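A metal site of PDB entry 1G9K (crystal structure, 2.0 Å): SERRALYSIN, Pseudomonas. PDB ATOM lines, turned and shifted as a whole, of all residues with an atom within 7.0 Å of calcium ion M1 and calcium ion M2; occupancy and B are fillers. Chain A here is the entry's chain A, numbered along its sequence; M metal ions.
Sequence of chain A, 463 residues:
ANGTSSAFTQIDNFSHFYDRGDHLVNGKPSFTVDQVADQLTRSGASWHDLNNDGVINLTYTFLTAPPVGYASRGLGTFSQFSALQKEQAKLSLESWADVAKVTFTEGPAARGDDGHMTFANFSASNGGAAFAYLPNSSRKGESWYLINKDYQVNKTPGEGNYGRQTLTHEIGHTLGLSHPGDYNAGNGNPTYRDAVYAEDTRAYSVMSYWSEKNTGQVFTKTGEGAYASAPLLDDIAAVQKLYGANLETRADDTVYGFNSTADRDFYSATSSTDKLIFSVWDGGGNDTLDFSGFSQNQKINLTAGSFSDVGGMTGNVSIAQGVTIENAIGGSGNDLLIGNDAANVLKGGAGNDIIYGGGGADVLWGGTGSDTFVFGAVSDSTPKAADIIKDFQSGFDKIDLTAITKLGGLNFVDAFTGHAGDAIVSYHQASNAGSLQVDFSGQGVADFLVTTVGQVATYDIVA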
ATOM      1  N   PHE A 294      10.740 -35.023  -0.322  1.00  0.00           N
ATOM      2  CA  PHE A 294       9.651 -34.671   0.580  1.00  0.00           C
ATOM      3  C   PHE A 294       9.596 -33.171   0.891  1.00  0.00           C
ATOM      4  O   PHE A 294      10.639 -32.507   0.939  1.00  0.00           O
ATOM      5  CB  PHE A 294       9.785 -35.458   1.893  1.00  0.00           C
ATOM      6  CG  PHE A 294       9.521 -36.926   1.751  1.00  0.00           C
ATOM      7  CD1 PHE A 294       8.311 -37.389   1.229  1.00  0.00           C
ATOM      8  CD2 PHE A 294      10.471 -37.860   2.141  1.00  0.00           C
ATOM      9  CE1 PHE A 294       8.052 -38.749   1.114  1.00  0.00           C
ATOM     10  CE2 PHE A 294      10.226 -39.230   2.028  1.00  0.00           C
ATOM     11  CZ  PHE A 294       9.014 -39.674   1.510  1.00  0.00           C
ATOM     12  N   GLN A 296       7.504 -32.111   3.579  1.00  0.00           N
ATOM     13  CA  GLN A 296       7.117 -32.011   4.989  1.00  0.00           C
ATOM     14  C   GLN A 296       8.353 -31.807   5.856  1.00  0.00           C
ATOM     15  O   GLN A 296       9.470 -32.096   5.426  1.00  0.00           O
ATOM     16  CB  GLN A 296       6.390 -33.289   5.446  1.00  0.00           C
ATOM     17  CG  GLN A 296       5.196 -33.705   4.583  1.00  0.00           C
ATOM     18  CD  GLN A 296       5.583 -34.647   3.456  1.00  0.00           C
ATOM     19  OE1 GLN A 296       6.683 -34.579   2.918  1.00  0.00           O
ATOM     20  NE2 GLN A 296       4.660 -35.534   3.085  1.00  0.00           N
ATOM     21  N   GLN A 298      11.086 -32.717   8.324  1.00  0.00           N
ATOM     22  CA  GLN A 298      11.632 -34.015   8.721  1.00  0.00           C
ATOM     23  C   GLN A 298      12.714 -33.864   9.785  1.00  0.00           C
ATOM     24  O   GLN A 298      13.257 -32.781   9.984  1.00  0.00           O
ATOM     25  CB  GLN A 298      12.215 -34.729   7.504  1.00  0.00           C
ATOM     26  CG  GLN A 298      11.304 -34.725   6.295  1.00  0.00           C
ATOM     27  CD  GLN A 298      11.913 -35.474   5.116  1.00  0.00           C
ATOM     28  OE1 GLN A 298      11.817 -36.694   5.039  1.00  0.00           O
ATOM     29  NE2 GLN A 298      12.554 -34.740   4.212  1.00  0.00           N
ATOM     30  N   GLY A 330      18.122 -33.579   3.317  1.00  0.00           N
ATOM     31  CA  GLY A 330      16.786 -33.197   3.750  1.00  0.00           C
ATOM     32  C   GLY A 330      15.901 -32.818   2.572  1.00  0.00           C
ATOM     33  O   GLY A 330      16.299 -32.948   1.426  1.00  0.00           O
ATOM     34  N   GLY A 331      14.693 -32.360   2.881  1.00  0.00           N
ATOM     35  CA  GLY A 331      13.757 -31.971   1.834  1.00  0.00           C
ATOM     36  C   GLY A 331      13.507 -30.471   1.792  1.00  0.00           C
ATOM     37  O   GLY A 331      14.308 -29.685   2.313  1.00  0.00           O
ATOM     38  N   SER A 332      12.393 -30.062   1.193  1.00  0.00           N
ATOM     39  CA  SER A 332      12.082 -28.647   1.089  1.00  0.00           C
ATOM     40  C   SER A 332      11.476 -28.080   2.365  1.00  0.00           C
ATOM     41  O   SER A 332      11.193 -26.883   2.442  1.00  0.00           O
ATOM     42  CB  SER A 332      11.141 -28.396  -0.089  1.00  0.00           C
ATOM     43  OG  SER A 332       9.906 -29.070   0.086  1.00  0.00           O
ATOM     44  N   GLY A 333      11.289 -28.927   3.368  1.00  0.00           N
ATOM     45  CA  GLY A 333      10.731 -28.453   4.616  1.00  0.00           C
ATOM     46  C   GLY A 333      11.810 -28.010   5.600  1.00  0.00           C
ATOM     47  O   GLY A 333      12.997 -28.069   5.282  1.00  0.00           O
ATOM     48  N   ASN A 334      11.395 -27.571   6.780  1.00  0.00           N
ATOM     49  CA  ASN A 334      12.313 -27.133   7.824  1.00  0.00           C
ATOM     50  C   ASN A 334      12.711 -28.401   8.575  1.00  0.00           C
ATOM     51  O   ASN A 334      11.947 -28.906   9.406  1.00  0.00           O
ATOM     52  CB  ASN A 334      11.618 -26.148   8.753  1.00  0.00           C
ATOM     53  CG  ASN A 334      10.958 -25.014   7.994  1.00  0.00           C
ATOM     54  OD1 ASN A 334      11.548 -24.418   7.095  1.00  0.00           O
ATOM     55  ND2 ASN A 334       9.726 -24.702   8.361  1.00  0.00           N
ATOM     56  N   ASP A 335      13.892 -28.916   8.282  1.00  0.00           N
ATOM     57  CA  ASP A 335      14.352 -30.166   8.867  1.00  0.00           C
ATOM     58  C   ASP A 335      15.443 -30.074   9.928  1.00  0.00           C
ATOM     59  O   ASP A 335      16.095 -29.048  10.097  1.00  0.00           O
ATOM     60  CB  ASP A 335      14.862 -31.079   7.749  1.00  0.00           C
ATOM     61  CG  ASP A 335      14.017 -30.999   6.494  1.00  0.00           C
ATOM     62  OD1 ASP A 335      12.794 -31.193   6.577  1.00  0.00           O
ATOM     63  OD2 ASP A 335      14.588 -30.747   5.407  1.00  0.00           O
ATOM     64  N   LEU A 336      15.611 -31.175  10.664  1.00  0.00           N
ATOM     65  CA  LEU A 336      16.661 -31.269  11.663  1.00  0.00           C
ATOM     66  C   LEU A 336      17.538 -32.409  11.138  1.00  0.00           C
ATOM     67  O   LEU A 336      17.025 -33.464  10.757  1.00  0.00           O
ATOM     68  CB  LEU A 336      16.104 -31.647  13.031  1.00  0.00           C
ATOM     69  CG  LEU A 336      15.104 -30.698  13.693  1.00  0.00           C
ATOM     70  CD1 LEU A 336      14.766 -31.225  15.085  1.00  0.00           C
ATOM     71  CD2 LEU A 336      15.682 -29.295  13.786  1.00  0.00           C
ATOM     72  N   LEU A 337      18.843 -32.181  11.075  1.00  0.00           N
ATOM     73  CA  LEU A 337      19.743 -33.229  10.610  1.00  0.00           C
ATOM     74  C   LEU A 337      20.821 -33.439  11.644  1.00  0.00           C
ATOM     75  O   LEU A 337      21.575 -32.520  11.983  1.00  0.00           O
ATOM     76  CB  LEU A 337      20.383 -32.878   9.262  1.00  0.00           C
ATOM     77  CG  LEU A 337      19.514 -32.932   8.000  1.00  0.00           C
ATOM     78  CD1 LEU A 337      18.640 -31.699   7.946  1.00  0.00           C
ATOM     79  CD2 LEU A 337      20.409 -32.991   6.766  1.00  0.00           C
ATOM     80  N   LYS A 347      22.969 -32.184   3.888  1.00  0.00           N
ATOM     81  CA  LYS A 347      22.343 -31.138   3.074  1.00  0.00           C
ATOM     82  C   LYS A 347      20.907 -30.898   3.504  1.00  0.00           C
ATOM     83  O   LYS A 347      20.060 -31.794   3.422  1.00  0.00           O
ATOM     84  CB  LYS A 347      22.381 -31.551   1.595  1.00  0.00           C
ATOM     85  CG  LYS A 347      23.776 -31.828   1.068  1.00  0.00           C
ATOM     86  CD  LYS A 347      23.774 -32.034  -0.439  1.00  0.00           C
ATOM     87  CE  LYS A 347      25.195 -32.140  -0.988  1.00  0.00           C
ATOM     88  NZ  LYS A 347      25.201 -32.240  -2.461  1.00  0.00           N
ATOM     89  N   GLY A 348      20.616 -29.683   3.962  1.00  0.00           N
ATOM     90  CA  GLY A 348      19.275 -29.356   4.412  1.00  0.00           C
ATOM     91  C   GLY A 348      18.256 -29.086   3.310  1.00  0.00           C
ATOM     92  O   GLY A 348      17.057 -29.252   3.521  1.00  0.00           O
ATOM     93  N   GLY A 349      18.736 -28.663   2.147  1.00  0.00           N
ATOM     94  CA  GLY A 349      17.825 -28.354   1.052  1.00  0.00           C
ATOM     95  C   GLY A 349      17.089 -27.064   1.345  1.00  0.00           C
ATOM     96  O   GLY A 349      17.524 -26.270   2.182  1.00  0.00           O
ATOM     97  N   ALA A 350      15.965 -26.857   0.674  1.00  0.00           N
ATOM     98  CA  ALA A 350      15.173 -25.650   0.892  1.00  0.00           C
ATOM     99  C   ALA A 350      14.672 -25.638   2.336  1.00  0.00           C
ATOM    100  O   ALA A 350      14.799 -26.627   3.053  1.00  0.00           O
ATOM    101  CB  ALA A 350      14.002 -25.604  -0.073  1.00  0.00           C
ATOM    102  N   GLY A 351      14.098 -24.513   2.758  1.00  0.00           N
ATOM    103  CA  GLY A 351      13.594 -24.413   4.114  1.00  0.00           C
ATOM    104  C   GLY A 351      14.666 -24.047   5.124  1.00  0.00           C
ATOM    105  O   GLY A 351      15.868 -24.120   4.831  1.00  0.00           O
ATOM    106  N   ASN A 352      14.224 -23.665   6.320  1.00  0.00           N
ATOM    107  CA  ASN A 352      15.125 -23.287   7.399  1.00  0.00           C
ATOM    108  C   ASN A 352      15.475 -24.518   8.203  1.00  0.00           C
ATOM    109  O   ASN A 352      14.698 -24.982   9.024  1.00  0.00           O
ATOM    110  CB  ASN A 352      14.461 -22.242   8.298  1.00  0.00           C
ATOM    111  CG  ASN A 352      13.957 -21.048   7.512  1.00  0.00           C
ATOM    112  OD1 ASN A 352      14.415 -20.781   6.405  1.00  0.00           O
ATOM    113  ND2 ASN A 352      13.016 -20.314   8.099  1.00  0.00           N
ATOM    114  N   ASP A 353      16.666 -25.050   7.948  1.00  0.00           N
ATOM    115  CA  ASP A 353      17.131 -26.262   8.604  1.00  0.00           C
ATOM    116  C   ASP A 353      18.126 -26.041   9.746  1.00  0.00           C
ATOM    117  O   ASP A 353      18.815 -25.021   9.804  1.00  0.00           O
ATOM    118  CB  ASP A 353      17.762 -27.167   7.549  1.00  0.00           C
ATOM    119  CG  ASP A 353      16.864 -27.366   6.337  1.00  0.00           C
ATOM    120  OD1 ASP A 353      15.779 -27.963   6.503  1.00  0.00           O
ATOM    121  OD2 ASP A 353      17.235 -26.923   5.234  1.00  0.00           O
ATOM    122  N   ILE A 355      21.247 -28.014  11.388  1.00  0.00           N
ATOM    123  CA  ILE A 355      22.182 -29.100  11.137  1.00  0.00           C
ATOM    124  C   ILE A 355      23.220 -29.277  12.243  1.00  0.00           C
ATOM    125  O   ILE A 355      23.780 -28.306  12.757  1.00  0.00           O
ATOM    126  CB  ILE A 355      22.894 -28.855   9.782  1.00  0.00           C
ATOM    127  CG1 ILE A 355      21.840 -28.710   8.679  1.00  0.00           C
ATOM    128  CG2 ILE A 355      23.847 -30.006   9.455  1.00  0.00           C
ATOM    129  CD1 ILE A 355      22.406 -28.335   7.328  1.00  0.00           C
ATOM    130  N   TRP A 365      25.878 -28.455   4.054  1.00  0.00           N
ATOM    131  CA  TRP A 365      25.214 -27.676   3.016  1.00  0.00           C
ATOM    132  C   TRP A 365      23.863 -27.239   3.578  1.00  0.00           C
ATOM    133  O   TRP A 365      23.010 -28.082   3.848  1.00  0.00           O
ATOM    134  CB  TRP A 365      24.968 -28.506   1.768  1.00  0.00           C
ATOM    135  CG  TRP A 365      26.185 -28.945   1.048  1.00  0.00           C
ATOM    136  CD1 TRP A 365      26.964 -30.027   1.334  1.00  0.00           C
ATOM    137  CD2 TRP A 365      26.757 -28.331  -0.111  1.00  0.00           C
ATOM    138  NE1 TRP A 365      27.987 -30.126   0.413  1.00  0.00           N
ATOM    139  CE2 TRP A 365      27.880 -29.101  -0.480  1.00  0.00           C
ATOM    140  CE3 TRP A 365      26.425 -27.198  -0.870  1.00  0.00           C
ATOM    141  CZ2 TRP A 365      28.678 -28.775  -1.583  1.00  0.00           C
ATOM    142  CZ3 TRP A 365      27.218 -26.875  -1.961  1.00  0.00           C
ATOM    143  CH2 TRP A 365      28.329 -27.660  -2.314  1.00  0.00           C
ATOM    144  N   GLY A 366      23.679 -25.940   3.756  1.00  0.00           N
ATOM    145  CA  GLY A 366      22.418 -25.458   4.289  1.00  0.00           C
ATOM    146  C   GLY A 366      21.336 -25.346   3.230  1.00  0.00           C
ATOM    147  O   GLY A 366      20.142 -25.417   3.532  1.00  0.00           O
ATOM    148  N   GLY A 367      21.755 -25.197   1.978  1.00  0.00           N
ATOM    149  CA  GLY A 367      20.801 -25.057   0.892  1.00  0.00           C
ATOM    150  C   GLY A 367      20.195 -23.657   0.940  1.00  0.00           C
ATOM    151  O   GLY A 367      20.788 -22.757   1.518  1.00  0.00           O
ATOM    152  N   THR A 368      19.015 -23.481   0.351  1.00  0.00           N
ATOM    153  CA  THR A 368      18.360 -22.182   0.375  1.00  0.00           C
ATOM    154  C   THR A 368      17.657 -22.006   1.721  1.00  0.00           C
ATOM    155  O   THR A 368      17.459 -22.974   2.451  1.00  0.00           O
ATOM    156  CB  THR A 368      17.339 -22.045  -0.780  1.00  0.00           C
ATOM    157  OG1 THR A 368      16.324 -23.040  -0.642  1.00  0.00           O
ATOM    158  CG2 THR A 368      18.027 -22.202  -2.127  1.00  0.00           C
ATOM    159  N   GLY A 369      17.274 -20.764   2.049  1.00  0.00           N
ATOM    160  CA  GLY A 369      16.598 -20.486   3.306  1.00  0.00           C
ATOM    161  C   GLY A 369      17.566 -20.054   4.403  1.00  0.00           C
ATOM    162  O   GLY A 369      18.766 -19.899   4.145  1.00  0.00           O
ATOM    163  N   SER A 370      17.049 -19.844   5.612  1.00  0.00           N
ATOM    164  CA  SER A 370      17.885 -19.442   6.751  1.00  0.00           C
ATOM    165  C   SER A 370      18.195 -20.689   7.561  1.00  0.00           C
ATOM    166  O   SER A 370      17.344 -21.210   8.277  1.00  0.00           O
ATOM    167  CB  SER A 370      17.177 -18.417   7.624  1.00  0.00           C
ATOM    168  OG  SER A 370      16.987 -17.213   6.927  1.00  0.00           O
ATOM    169  N   ASP A 371      19.443 -21.151   7.447  1.00  0.00           N
ATOM    170  CA  ASP A 371      19.872 -22.360   8.122  1.00  0.00           C
ATOM    171  C   ASP A 371      20.794 -22.133   9.303  1.00  0.00           C
ATOM    172  O   ASP A 371      21.565 -21.183   9.341  1.00  0.00           O
ATOM    173  CB  ASP A 371      20.529 -23.269   7.099  1.00  0.00           C
ATOM    174  CG  ASP A 371      19.589 -23.607   5.955  1.00  0.00           C
ATOM    175  OD1 ASP A 371      18.574 -24.287   6.209  1.00  0.00           O
ATOM    176  OD2 ASP A 371      19.849 -23.176   4.806  1.00  0.00           O
ATOM    177  N   ASP A 391      28.218 -23.505   1.699  1.00  0.00           N
ATOM    178  CA  ASP A 391      27.342 -22.482   1.148  1.00  0.00           C
ATOM    179  C   ASP A 391      26.799 -21.494   2.181  1.00  0.00           C
ATOM    180  O   ASP A 391      25.664 -21.028   2.067  1.00  0.00           O
ATOM    181  CB  ASP A 391      26.172 -23.144   0.405  1.00  0.00           C
ATOM    182  CG  ASP A 391      25.254 -23.939   1.342  1.00  0.00           C
ATOM    183  OD1 ASP A 391      25.665 -24.286   2.463  1.00  0.00           O
ATOM    184  OD2 ASP A 391      24.110 -24.233   0.925  1.00  0.00           O
ATOM    185  N   ASP A 397      22.184 -17.236   7.478  1.00  0.00           N
ATOM    186  CA  ASP A 397      22.549 -18.427   8.235  1.00  0.00           C
ATOM    187  C   ASP A 397      23.202 -18.057   9.565  1.00  0.00           C
ATOM    188  O   ASP A 397      23.628 -16.912   9.756  1.00  0.00           O
ATOM    189  CB  ASP A 397      23.517 -19.312   7.440  1.00  0.00           C
ATOM    190  CG  ASP A 397      22.961 -19.719   6.087  1.00  0.00           C
ATOM    191  OD1 ASP A 397      21.725 -19.843   5.960  1.00  0.00           O
ATOM    192  OD2 ASP A 397      23.760 -19.927   5.153  1.00  0.00           O
HETATM  193 CA    CA M   1      17.955 -24.804   3.975  1.00  0.00          CA
HETATM  194 CA    CA M   2      15.022 -28.597   4.334  1.00  0.00          CA
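The backbone NH (N) of Gly 348 sits at hydrogen-bond distance from the backbone carbonyl oxygen (O) of Trp 365, 2.9 Å away.
The backbone NH (N) of Gly 366 lies within hydrogen-bond range of the side-chain carboxylate (OD1) of Asp 391 (2.9 Å).
The side-chain carboxylate (OD1) of Asp 397 is in hydrogen-bond range of the backbone NH (N) of Asp 371.
The side-chain amide nitrogen (NE2) of Gln 298 lies close to the backbone NH (N) of Gly 331, 3.5 Å away.
The side-chain carboxylate of Asp 335 is in hydrogen-bond range of the backbone NH of Gln 298 (2.9 Å).
N of Gly 367 lies within hydrogen-bond range of OD2 of Asp 391 (2.8 Å).
C of Gly 367 touches calcium ion M1 (3.9 Å).
The nearest printed residue that does not touch calcium ion M1 is Gly 348 (4.3 Å).
Seven residues have an atom within 4 Å of calcium ion M2: Gly 331, Gly 333, Asp 335, Gly 348, Gly 349, Ala 350 and Asp 353.
Along chain A the residues within 4 Å of calcium ion M2 span positions 331 to 353.
The nearest printed residue that does not touch calcium ion M2 is Ser 332 (4.1 Å).
Calcium ion M1 is bound by O of Gly 366, O of Gly 349, O of Gly 351, OD1 of Asp 371, O of Thr 368, OD2 of Asp 353 and OD2 of Asp 371.
Calcium ion M1 has seven donor atoms within binding distance.
Calcium ion M2 is bound by the backbone carbonyl oxygen of Gly 348 (2.3 Å), the backbone carbonyl oxygen of Gly 333 (2.3 Å), the backbone carbonyl oxygen of Ala 350 (2.4 Å), the side-chain carboxylate of Asp 353 (2.4 Å), the backbone carbonyl oxygen of Gly 331 (2.4 Å) and the side-chain carboxylate of Asp 335 (2.4 Å).
Slightly farther from calcium ion M2 lies OD2 of Asp 353 (2.9 Å).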
